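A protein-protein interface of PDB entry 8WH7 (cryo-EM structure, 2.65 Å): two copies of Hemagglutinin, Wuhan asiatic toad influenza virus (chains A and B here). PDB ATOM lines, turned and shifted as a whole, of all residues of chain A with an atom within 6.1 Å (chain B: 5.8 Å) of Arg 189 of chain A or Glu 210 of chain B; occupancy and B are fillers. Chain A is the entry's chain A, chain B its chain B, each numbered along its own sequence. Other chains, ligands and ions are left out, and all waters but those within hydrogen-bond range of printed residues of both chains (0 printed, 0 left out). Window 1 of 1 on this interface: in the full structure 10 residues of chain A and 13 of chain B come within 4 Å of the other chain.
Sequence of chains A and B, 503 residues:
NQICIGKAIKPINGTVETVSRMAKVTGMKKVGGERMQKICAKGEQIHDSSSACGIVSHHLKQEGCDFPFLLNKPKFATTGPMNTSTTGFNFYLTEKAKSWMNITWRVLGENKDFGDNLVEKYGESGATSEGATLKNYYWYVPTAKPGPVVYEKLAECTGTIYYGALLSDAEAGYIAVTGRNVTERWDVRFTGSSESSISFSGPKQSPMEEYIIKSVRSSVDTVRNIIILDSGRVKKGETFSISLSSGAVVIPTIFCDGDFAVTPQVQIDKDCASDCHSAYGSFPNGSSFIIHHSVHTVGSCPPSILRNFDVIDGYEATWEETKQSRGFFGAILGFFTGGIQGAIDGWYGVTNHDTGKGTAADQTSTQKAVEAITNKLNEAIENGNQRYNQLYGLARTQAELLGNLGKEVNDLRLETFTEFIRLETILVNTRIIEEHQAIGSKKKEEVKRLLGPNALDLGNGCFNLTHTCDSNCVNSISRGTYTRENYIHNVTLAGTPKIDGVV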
ATOM      1  N   VAL A 150       0.219  24.661  12.274  1.00  0.00           N
ATOM      2  CA  VAL A 150      -0.002  25.898  11.536  1.00  0.00           C
ATOM      3  C   VAL A 150       1.306  26.284  10.864  1.00  0.00           C
ATOM      4  O   VAL A 150       2.347  26.362  11.524  1.00  0.00           O
ATOM      5  CB  VAL A 150      -0.495  27.032  12.453  1.00  0.00           C
ATOM      6  CG1 VAL A 150      -0.503  28.347  11.705  1.00  0.00           C
ATOM      7  CG2 VAL A 150      -1.879  26.715  12.985  1.00  0.00           C
ATOM      8  N   TYR A 163      -4.986  24.478  -2.669  1.00  0.00           N
ATOM      9  CA  TYR A 163      -4.859  23.590  -1.521  1.00  0.00           C
ATOM     10  C   TYR A 163      -6.140  22.785  -1.373  1.00  0.00           C
ATOM     11  O   TYR A 163      -7.193  23.165  -1.887  1.00  0.00           O
ATOM     12  CB  TYR A 163      -4.580  24.375  -0.236  1.00  0.00           C
ATOM     13  CG  TYR A 163      -5.763  25.190   0.225  1.00  0.00           C
ATOM     14  CD1 TYR A 163      -6.120  26.359  -0.426  1.00  0.00           C
ATOM     15  CD2 TYR A 163      -6.531  24.784   1.305  1.00  0.00           C
ATOM     16  CE1 TYR A 163      -7.201  27.102  -0.014  1.00  0.00           C
ATOM     17  CE2 TYR A 163      -7.615  25.522   1.724  1.00  0.00           C
ATOM     18  CZ  TYR A 163      -7.945  26.680   1.059  1.00  0.00           C
ATOM     19  OH  TYR A 163      -9.025  27.420   1.472  1.00  0.00           O
ATOM     20  N   ASP A 187     -12.180  20.749   9.118  1.00  0.00           N
ATOM     21  CA  ASP A 187     -12.019  21.827   8.156  1.00  0.00           C
ATOM     22  C   ASP A 187     -10.548  22.108   7.890  1.00  0.00           C
ATOM     23  O   ASP A 187      -9.670  21.798   8.697  1.00  0.00           O
ATOM     24  CB  ASP A 187     -12.691  23.116   8.641  1.00  0.00           C
ATOM     25  CG  ASP A 187     -14.171  22.944   8.883  1.00  0.00           C
ATOM     26  OD1 ASP A 187     -14.758  21.996   8.324  1.00  0.00           O
ATOM     27  OD2 ASP A 187     -14.751  23.759   9.632  1.00  0.00           O
ATOM     28  N   VAL A 188     -10.300  22.706   6.728  1.00  0.00           N
ATOM     29  CA  VAL A 188      -9.006  23.268   6.364  1.00  0.00           C
ATOM     30  C   VAL A 188      -9.229  24.726   5.995  1.00  0.00           C
ATOM     31  O   VAL A 188     -10.105  25.036   5.177  1.00  0.00           O
ATOM     32  CB  VAL A 188      -8.350  22.501   5.203  1.00  0.00           C
ATOM     33  CG1 VAL A 188      -7.004  23.106   4.865  1.00  0.00           C
ATOM     34  CG2 VAL A 188      -8.199  21.035   5.555  1.00  0.00           C
ATOM     35  N   ARG A 189      -8.445  25.618   6.598  1.00  0.00           N
ATOM     36  CA  ARG A 189      -8.632  27.056   6.464  1.00  0.00           C
ATOM     37  C   ARG A 189      -7.373  27.714   5.925  1.00  0.00           C
ATOM     38  O   ARG A 189      -6.255  27.316   6.266  1.00  0.00           O
ATOM     39  CB  ARG A 189      -9.000  27.694   7.803  1.00  0.00           C
ATOM     40  CG  ARG A 189     -10.129  27.001   8.531  1.00  0.00           C
ATOM     41  CD  ARG A 189     -10.864  27.966   9.438  1.00  0.00           C
ATOM     42  NE  ARG A 189     -12.209  27.498   9.746  1.00  0.00           N
ATOM     43  CZ  ARG A 189     -12.916  27.895  10.793  1.00  0.00           C
ATOM     44  NH1 ARG A 189     -12.436  28.773  11.657  1.00  0.00           N
ATOM     45  NH2 ARG A 189     -14.134  27.397  10.980  1.00  0.00           N
ATOM     46  N   PHE A 190      -7.562  28.732   5.090  1.00  0.00           N
ATOM     47  CA  PHE A 190      -6.475  29.505   4.510  1.00  0.00           C
ATOM     48  C   PHE A 190      -6.724  30.976   4.796  1.00  0.00           C
ATOM     49  O   PHE A 190      -7.792  31.503   4.464  1.00  0.00           O
ATOM     50  CB  PHE A 190      -6.373  29.260   3.000  1.00  0.00           C
ATOM     51  CG  PHE A 190      -5.283  30.042   2.324  1.00  0.00           C
ATOM     52  CD1 PHE A 190      -5.525  31.308   1.822  1.00  0.00           C
ATOM     53  CD2 PHE A 190      -4.020  29.501   2.171  1.00  0.00           C
ATOM     54  CE1 PHE A 190      -4.528  32.022   1.196  1.00  0.00           C
ATOM     55  CE2 PHE A 190      -3.020  30.213   1.544  1.00  0.00           C
ATOM     56  CZ  PHE A 190      -3.274  31.473   1.057  1.00  0.00           C
ATOM     57  N   THR A 191      -5.744  31.634   5.408  1.00  0.00           N
ATOM     58  CA  THR A 191      -5.826  33.055   5.715  1.00  0.00           C
ATOM     59  C   THR A 191      -4.647  33.779   5.078  1.00  0.00           C
ATOM     60  O   THR A 191      -3.487  33.419   5.306  1.00  0.00           O
ATOM     61  CB  THR A 191      -5.886  33.295   7.229  1.00  0.00           C
ATOM     62  OG1 THR A 191      -6.023  34.697   7.492  1.00  0.00           O
ATOM     63  CG2 THR A 191      -4.663  32.739   7.949  1.00  0.00           C
ATOM     64  N   GLU A 195      -9.810  35.306   3.256  1.00  0.00           N
ATOM     65  CA  GLU A 195     -10.051  34.129   4.079  1.00  0.00           C
ATOM     66  C   GLU A 195     -10.855  33.104   3.294  1.00  0.00           C
ATOM     67  O   GLU A 195     -11.739  33.466   2.511  1.00  0.00           O
ATOM     68  CB  GLU A 195     -10.791  34.508   5.367  1.00  0.00           C
ATOM     69  CG  GLU A 195     -10.494  33.602   6.547  1.00  0.00           C
ATOM     70  CD  GLU A 195     -11.527  32.509   6.716  1.00  0.00           C
ATOM     71  OE1 GLU A 195     -12.669  32.690   6.242  1.00  0.00           O
ATOM     72  OE2 GLU A 195     -11.201  31.469   7.328  1.00  0.00           O
ATOM     73  N   SER A 196     -10.544  31.824   3.499  1.00  0.00           N
ATOM     74  CA  SER A 196     -11.263  30.750   2.824  1.00  0.00           C
ATOM     75  C   SER A 196     -11.198  29.491   3.674  1.00  0.00           C
ATOM     76  O   SER A 196     -10.331  29.349   4.537  1.00  0.00           O
ATOM     77  CB  SER A 196     -10.692  30.475   1.429  1.00  0.00           C
ATOM     78  OG  SER A 196     -10.478  31.678   0.713  1.00  0.00           O
ATOM     79  N   SER A 197     -12.117  28.564   3.409  1.00  0.00           N
ATOM     80  CA  SER A 197     -12.160  27.320   4.167  1.00  0.00           C
ATOM     81  C   SER A 197     -12.889  26.253   3.364  1.00  0.00           C
ATOM     82  O   SER A 197     -13.602  26.549   2.402  1.00  0.00           O
ATOM     83  CB  SER A 197     -12.838  27.517   5.525  1.00  0.00           C
ATOM     84  OG  SER A 197     -14.046  28.241   5.388  1.00  0.00           O
ATOM     85  N   ILE A 198     -12.694  25.002   3.779  1.00  0.00           N
ATOM     86  CA  ILE A 198     -13.364  23.861   3.163  1.00  0.00           C
ATOM     87  C   ILE A 198     -13.527  22.776   4.219  1.00  0.00           C
ATOM     88  O   ILE A 198     -12.746  22.693   5.171  1.00  0.00           O
ATOM     89  CB  ILE A 198     -12.589  23.351   1.926  1.00  0.00           C
ATOM     90  CG1 ILE A 198     -13.421  22.339   1.139  1.00  0.00           C
ATOM     91  CG2 ILE A 198     -11.257  22.753   2.334  1.00  0.00           C
ATOM     92  CD1 ILE A 198     -12.997  22.193  -0.299  1.00  0.00           C
ATOM     93  N   SER A 241      -0.678  32.066   6.172  1.00  0.00           N
ATOM     94  CA  SER A 241      -0.734  30.941   7.091  1.00  0.00           C
ATOM     95  C   SER A 241      -1.745  29.909   6.611  1.00  0.00           C
ATOM     96  O   SER A 241      -2.766  30.247   6.008  1.00  0.00           O
ATOM     97  CB  SER A 241      -1.104  31.404   8.501  1.00  0.00           C
ATOM     98  OG  SER A 241      -1.428  30.303   9.328  1.00  0.00           O
ATOM     99  N   ILE A 242      -1.443  28.642   6.887  1.00  0.00           N
ATOM    100  CA  ILE A 242      -2.299  27.515   6.534  1.00  0.00           C
ATOM    101  C   ILE A 242      -2.400  26.578   7.731  1.00  0.00           C
ATOM    102  O   ILE A 242      -1.395  26.286   8.389  1.00  0.00           O
ATOM    103  CB  ILE A 242      -1.770  26.747   5.304  1.00  0.00           C
ATOM    104  CG1 ILE A 242      -1.473  27.701   4.150  1.00  0.00           C
ATOM    105  CG2 ILE A 242      -2.768  25.693   4.865  1.00  0.00           C
ATOM    106  CD1 ILE A 242      -0.963  27.009   2.912  1.00  0.00           C
ATOM    107  N   SER A 243      -3.611  26.100   8.007  1.00  0.00           N
ATOM    108  CA  SER A 243      -3.837  25.118   9.059  1.00  0.00           C
ATOM    109  C   SER A 243      -3.821  23.719   8.457  1.00  0.00           C
ATOM    110  O   SER A 243      -4.575  23.435   7.522  1.00  0.00           O
ATOM    111  CB  SER A 243      -5.169  25.372   9.762  1.00  0.00           C
ATOM    112  OG  SER A 243      -5.178  26.639  10.390  1.00  0.00           O
ATOM    113  N   TYR B  92      -8.965  35.652  21.581  1.00  0.00           N
ATOM    114  CA  TYR B  92      -8.885  35.387  20.153  1.00  0.00           C
ATOM    115  C   TYR B  92      -9.935  36.213  19.420  1.00  0.00           C
ATOM    116  O   TYR B  92     -11.082  36.330  19.873  1.00  0.00           O
ATOM    117  CB  TYR B  92      -9.077  33.898  19.848  1.00  0.00           C
ATOM    118  CG  TYR B  92      -9.024  33.564  18.377  1.00  0.00           C
ATOM    119  CD1 TYR B  92      -7.812  33.379  17.733  1.00  0.00           C
ATOM    120  CD2 TYR B  92     -10.185  33.427  17.633  1.00  0.00           C
ATOM    121  CE1 TYR B  92      -7.757  33.073  16.390  1.00  0.00           C
ATOM    122  CE2 TYR B  92     -10.140  33.122  16.290  1.00  0.00           C
ATOM    123  CZ  TYR B  92      -8.924  32.945  15.675  1.00  0.00           C
ATOM    124  OH  TYR B  92      -8.877  32.640  14.336  1.00  0.00           O
ATOM    125  N   ARG B 185     -20.840  19.856  17.245  1.00  0.00           N
ATOM    126  CA  ARG B 185     -20.583  21.208  16.773  1.00  0.00           C
ATOM    127  C   ARG B 185     -21.805  22.058  17.075  1.00  0.00           C
ATOM    128  O   ARG B 185     -22.930  21.649  16.776  1.00  0.00           O
ATOM    129  CB  ARG B 185     -20.281  21.215  15.273  1.00  0.00           C
ATOM    130  CG  ARG B 185     -19.715  22.517  14.753  1.00  0.00           C
ATOM    131  CD  ARG B 185     -19.396  22.416  13.274  1.00  0.00           C
ATOM    132  NE  ARG B 185     -18.090  21.812  13.039  1.00  0.00           N
ATOM    133  CZ  ARG B 185     -17.288  22.130  12.034  1.00  0.00           C
ATOM    134  NH1 ARG B 185     -17.625  23.049  11.145  1.00  0.00           N
ATOM    135  NH2 ARG B 185     -16.116  21.513  11.918  1.00  0.00           N
ATOM    136  N   GLN B 205     -10.676  18.737  18.943  1.00  0.00           N
ATOM    137  CA  GLN B 205     -11.358  18.635  17.661  1.00  0.00           C
ATOM    138  C   GLN B 205     -11.262  19.976  16.951  1.00  0.00           C
ATOM    139  O   GLN B 205     -10.822  20.976  17.520  1.00  0.00           O
ATOM    140  CB  GLN B 205     -12.833  18.228  17.803  1.00  0.00           C
ATOM    141  CG  GLN B 205     -13.102  16.804  18.272  1.00  0.00           C
ATOM    142  CD  GLN B 205     -13.015  16.646  19.772  1.00  0.00           C
ATOM    143  OE1 GLN B 205     -13.058  17.625  20.513  1.00  0.00           O
ATOM    144  NE2 GLN B 205     -12.889  15.408  20.228  1.00  0.00           N
ATOM    145  N   PRO B 207     -13.072  23.275  15.133  1.00  0.00           N
ATOM    146  CA  PRO B 207     -11.944  24.179  14.898  1.00  0.00           C
ATOM    147  C   PRO B 207     -11.297  24.723  16.170  1.00  0.00           C
ATOM    148  O   PRO B 207     -10.536  25.683  16.092  1.00  0.00           O
ATOM    149  CB  PRO B 207     -12.587  25.313  14.106  1.00  0.00           C
ATOM    150  CG  PRO B 207     -13.994  25.365  14.617  1.00  0.00           C
ATOM    151  CD  PRO B 207     -14.346  24.011  15.185  1.00  0.00           C
ATOM    152  N   MET B 208     -11.597  24.121  17.321  1.00  0.00           N
ATOM    153  CA  MET B 208     -11.037  24.607  18.577  1.00  0.00           C
ATOM    154  C   MET B 208      -9.525  24.421  18.646  1.00  0.00           C
ATOM    155  O   MET B 208      -8.841  25.212  19.308  1.00  0.00           O
ATOM    156  CB  MET B 208     -11.717  23.902  19.749  1.00  0.00           C
ATOM    157  CG  MET B 208     -11.166  24.255  21.114  1.00  0.00           C
ATOM    158  SD  MET B 208     -11.968  25.714  21.804  1.00  0.00           S
ATOM    159  CE  MET B 208     -11.323  25.695  23.473  1.00  0.00           C
ATOM    160  N   GLU B 209      -8.992  23.406  17.963  1.00  0.00           N
ATOM    161  CA  GLU B 209      -7.550  23.184  17.958  1.00  0.00           C
ATOM    162  C   GLU B 209      -6.811  24.391  17.403  1.00  0.00           C
ATOM    163  O   GLU B 209      -5.773  24.796  17.941  1.00  0.00           O
ATOM    164  CB  GLU B 209      -7.218  21.943  17.136  1.00  0.00           C
ATOM    165  CG  GLU B 209      -7.584  20.635  17.797  1.00  0.00           C
ATOM    166  CD  GLU B 209      -7.811  19.530  16.787  1.00  0.00           C
ATOM    167  OE1 GLU B 209      -7.905  19.841  15.581  1.00  0.00           O
ATOM    168  OE2 GLU B 209      -7.897  18.354  17.197  1.00  0.00           O
ATOM    169  N   GLU B 210      -7.323  24.971  16.318  1.00  0.00           N
ATOM    170  CA  GLU B 210      -6.704  26.163  15.752  1.00  0.00           C
ATOM    171  C   GLU B 210      -6.824  27.357  16.692  1.00  0.00           C
ATOM    172  O   GLU B 210      -5.880  28.149  16.810  1.00  0.00           O
ATOM    173  CB  GLU B 210      -7.331  26.470  14.394  1.00  0.00           C
ATOM    174  CG  GLU B 210      -7.062  27.866  13.873  1.00  0.00           C
ATOM    175  CD  GLU B 210      -7.962  28.236  12.712  1.00  0.00           C
ATOM    176  OE1 GLU B 210      -8.806  27.403  12.323  1.00  0.00           O
ATOM    177  OE2 GLU B 210      -7.823  29.360  12.184  1.00  0.00           O
ATOM    178  N   TYR B 211      -7.965  27.497  17.371  1.00  0.00           N
ATOM    179  CA  TYR B 211      -8.134  28.592  18.319  1.00  0.00           C
ATOM    180  C   TYR B 211      -7.107  28.512  19.439  1.00  0.00           C
ATOM    181  O   TYR B 211      -6.539  29.532  19.844  1.00  0.00           O
ATOM    182  CB  TYR B 211      -9.545  28.577  18.905  1.00  0.00           C
ATOM    183  CG  TYR B 211     -10.645  28.853  17.909  1.00  0.00           C
ATOM    184  CD1 TYR B 211     -10.387  29.537  16.731  1.00  0.00           C
ATOM    185  CD2 TYR B 211     -11.944  28.435  18.151  1.00  0.00           C
ATOM    186  CE1 TYR B 211     -11.392  29.792  15.823  1.00  0.00           C
ATOM    187  CE2 TYR B 211     -12.954  28.685  17.249  1.00  0.00           C
ATOM    188  CZ  TYR B 211     -12.672  29.362  16.087  1.00  0.00           C
ATOM    189  OH  TYR B 211     -13.676  29.614  15.184  1.00  0.00           O
ATOM    190  N   ILE B 212      -6.860  27.308  19.957  1.00  0.00           N
ATOM    191  CA  ILE B 212      -5.890  27.160  21.040  1.00  0.00           C
ATOM    192  C   ILE B 212      -4.496  27.556  20.572  1.00  0.00           C
ATOM    193  O   ILE B 212      -3.747  28.220  21.297  1.00  0.00           O
ATOM    194  CB  ILE B 212      -5.917  25.723  21.590  1.00  0.00           C
ATOM    195  CG1 ILE B 212      -7.296  25.403  22.164  1.00  0.00           C
ATOM    196  CG2 ILE B 212      -4.849  25.541  22.648  1.00  0.00           C
ATOM    197  CD1 ILE B 212      -7.418  23.999  22.699  1.00  0.00           C
ATOM    198  N   ILE B 213      -4.123  27.155  19.356  1.00  0.00           N
ATOM    199  CA  ILE B 213      -2.775  27.422  18.865  1.00  0.00           C
ATOM    200  C   ILE B 213      -2.582  28.907  18.575  1.00  0.00           C
ATOM    201  O   ILE B 213      -1.533  29.480  18.889  1.00  0.00           O
ATOM    202  CB  ILE B 213      -2.482  26.560  17.625  1.00  0.00           C
ATOM    203  CG1 ILE B 213      -2.381  25.087  18.015  1.00  0.00           C
ATOM    204  CG2 ILE B 213      -1.202  27.009  16.951  1.00  0.00           C
ATOM    205  CD1 ILE B 213      -2.248  24.159  16.836  1.00  0.00           C
ATOM    206  N   LYS B 214      -3.581  29.554  17.983  1.00  0.00           N
ATOM    207  CA  LYS B 214      -3.428  30.926  17.512  1.00  0.00           C
ATOM    208  C   LYS B 214      -3.675  31.975  18.588  1.00  0.00           C
ATOM    209  O   LYS B 214      -3.596  33.171  18.288  1.00  0.00           O
ATOM    210  CB  LYS B 214      -4.371  31.185  16.337  1.00  0.00           C
ATOM    211  CG  LYS B 214      -3.917  30.588  15.023  1.00  0.00           C
ATOM    212  CD  LYS B 214      -4.979  30.785  13.960  1.00  0.00           C
ATOM    213  CE  LYS B 214      -4.478  30.387  12.588  1.00  0.00           C
ATOM    214  NZ  LYS B 214      -5.459  30.743  11.529  1.00  0.00           N
ATOM    215  N   SER B 215      -3.972  31.574  19.819  1.00  0.00           N
ATOM    216  CA  SER B 215      -4.341  32.536  20.845  1.00  0.00           C
ATOM    217  C   SER B 215      -3.132  33.343  21.310  1.00  0.00           C
ATOM    218  O   SER B 215      -1.977  32.997  21.046  1.00  0.00           O
ATOM    219  CB  SER B 215      -4.976  31.827  22.039  1.00  0.00           C
ATOM    220  OG  SER B 215      -3.994  31.157  22.805  1.00  0.00           O
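NH1 of Arg 185 of chain B is in salt-bridge range of OD2 of Asp 187 of chain A. The guanidinium group (NH1) of Arg 189 of chain A lies within salt-bridge range of the side-chain carboxylate (OE1) of Glu 210 of chain B (3.9 Å).
The side-chain carboxylate (OD2) of Asp 187 of chain A lies within salt-bridge range of the guanidinium group (NH2) of Arg 189 of chain A (3.9 Å). N of Ser 243 of chain A sits at hydrogen-bond distance from O of Arg 189 of chain A, 3.4 Å away. The side-chain carboxylate of Glu 210 of chain B lies within salt-bridge range of the side-chain amino group of Lys 214 of chain B, 2.8 Å away.
Among the printed residues, merely in contact across the chains: Arg 189 of chain A with Tyr 211 of chain B and Ser 243 of chain A with Glu 210 of chain B.
Of the printed residues of chain B, Asp 187 of chain A touches Arg 185. Of the printed residues of chain B, Arg 189 of chain A touches Glu 210 and Tyr 211. Ser 196 of chain A touches none of the printed residues of chain B. Of the printed residues of chain B, Ser 243 of chain A touches Glu 210 (3.96 Å). Of the printed residues of chain A, Arg 185 of chain B touches Asp 187 (3.3 Å). Glu 209 of chain B touches none of the printed residues of chain A. Of chain A, only Arg 189 (3.6 Å) and Ser 243 (3.96 Å) come within 4 Å of Glu 210 of chain B. Printed residues of chain A within 4 Å of Tyr 211 of chain B: Arg 189 (3.8 Å). The nearest residue of chain B that does not touch Arg 189 of chain A is Pro 207 of chain B (4.1 Å). The nearest residue of chain A that does not touch Glu 210 of chain B is Val 150 of chain A (5.4 Å). The nearest printed residue of chain A that does not touch Arg 185 of chain B is Arg 189 of chain A (5.6 Å).
Of the 12 printed residues of chain B, 3 touch a printed residue of chain A. Hydrophobic or aromatic side chains of chain B within 4 Å of the printed part of chain A: Tyr 211. Of the 14 printed residues of chain A, 3 touch a printed residue of chain B. Among the printed residues, Asp or Glu carboxylates within 4 Å of a Lys or Arg side-chain nitrogen of the other chain: Asp 187 of chain A with Arg 185 of chain B and Arg 189 of chain A with Glu 210 of chain B.
No position is printed for both chains. Of the 4 pairs that touch across the chains among the printed residues, none has its exchanged pair printed and touching as well.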
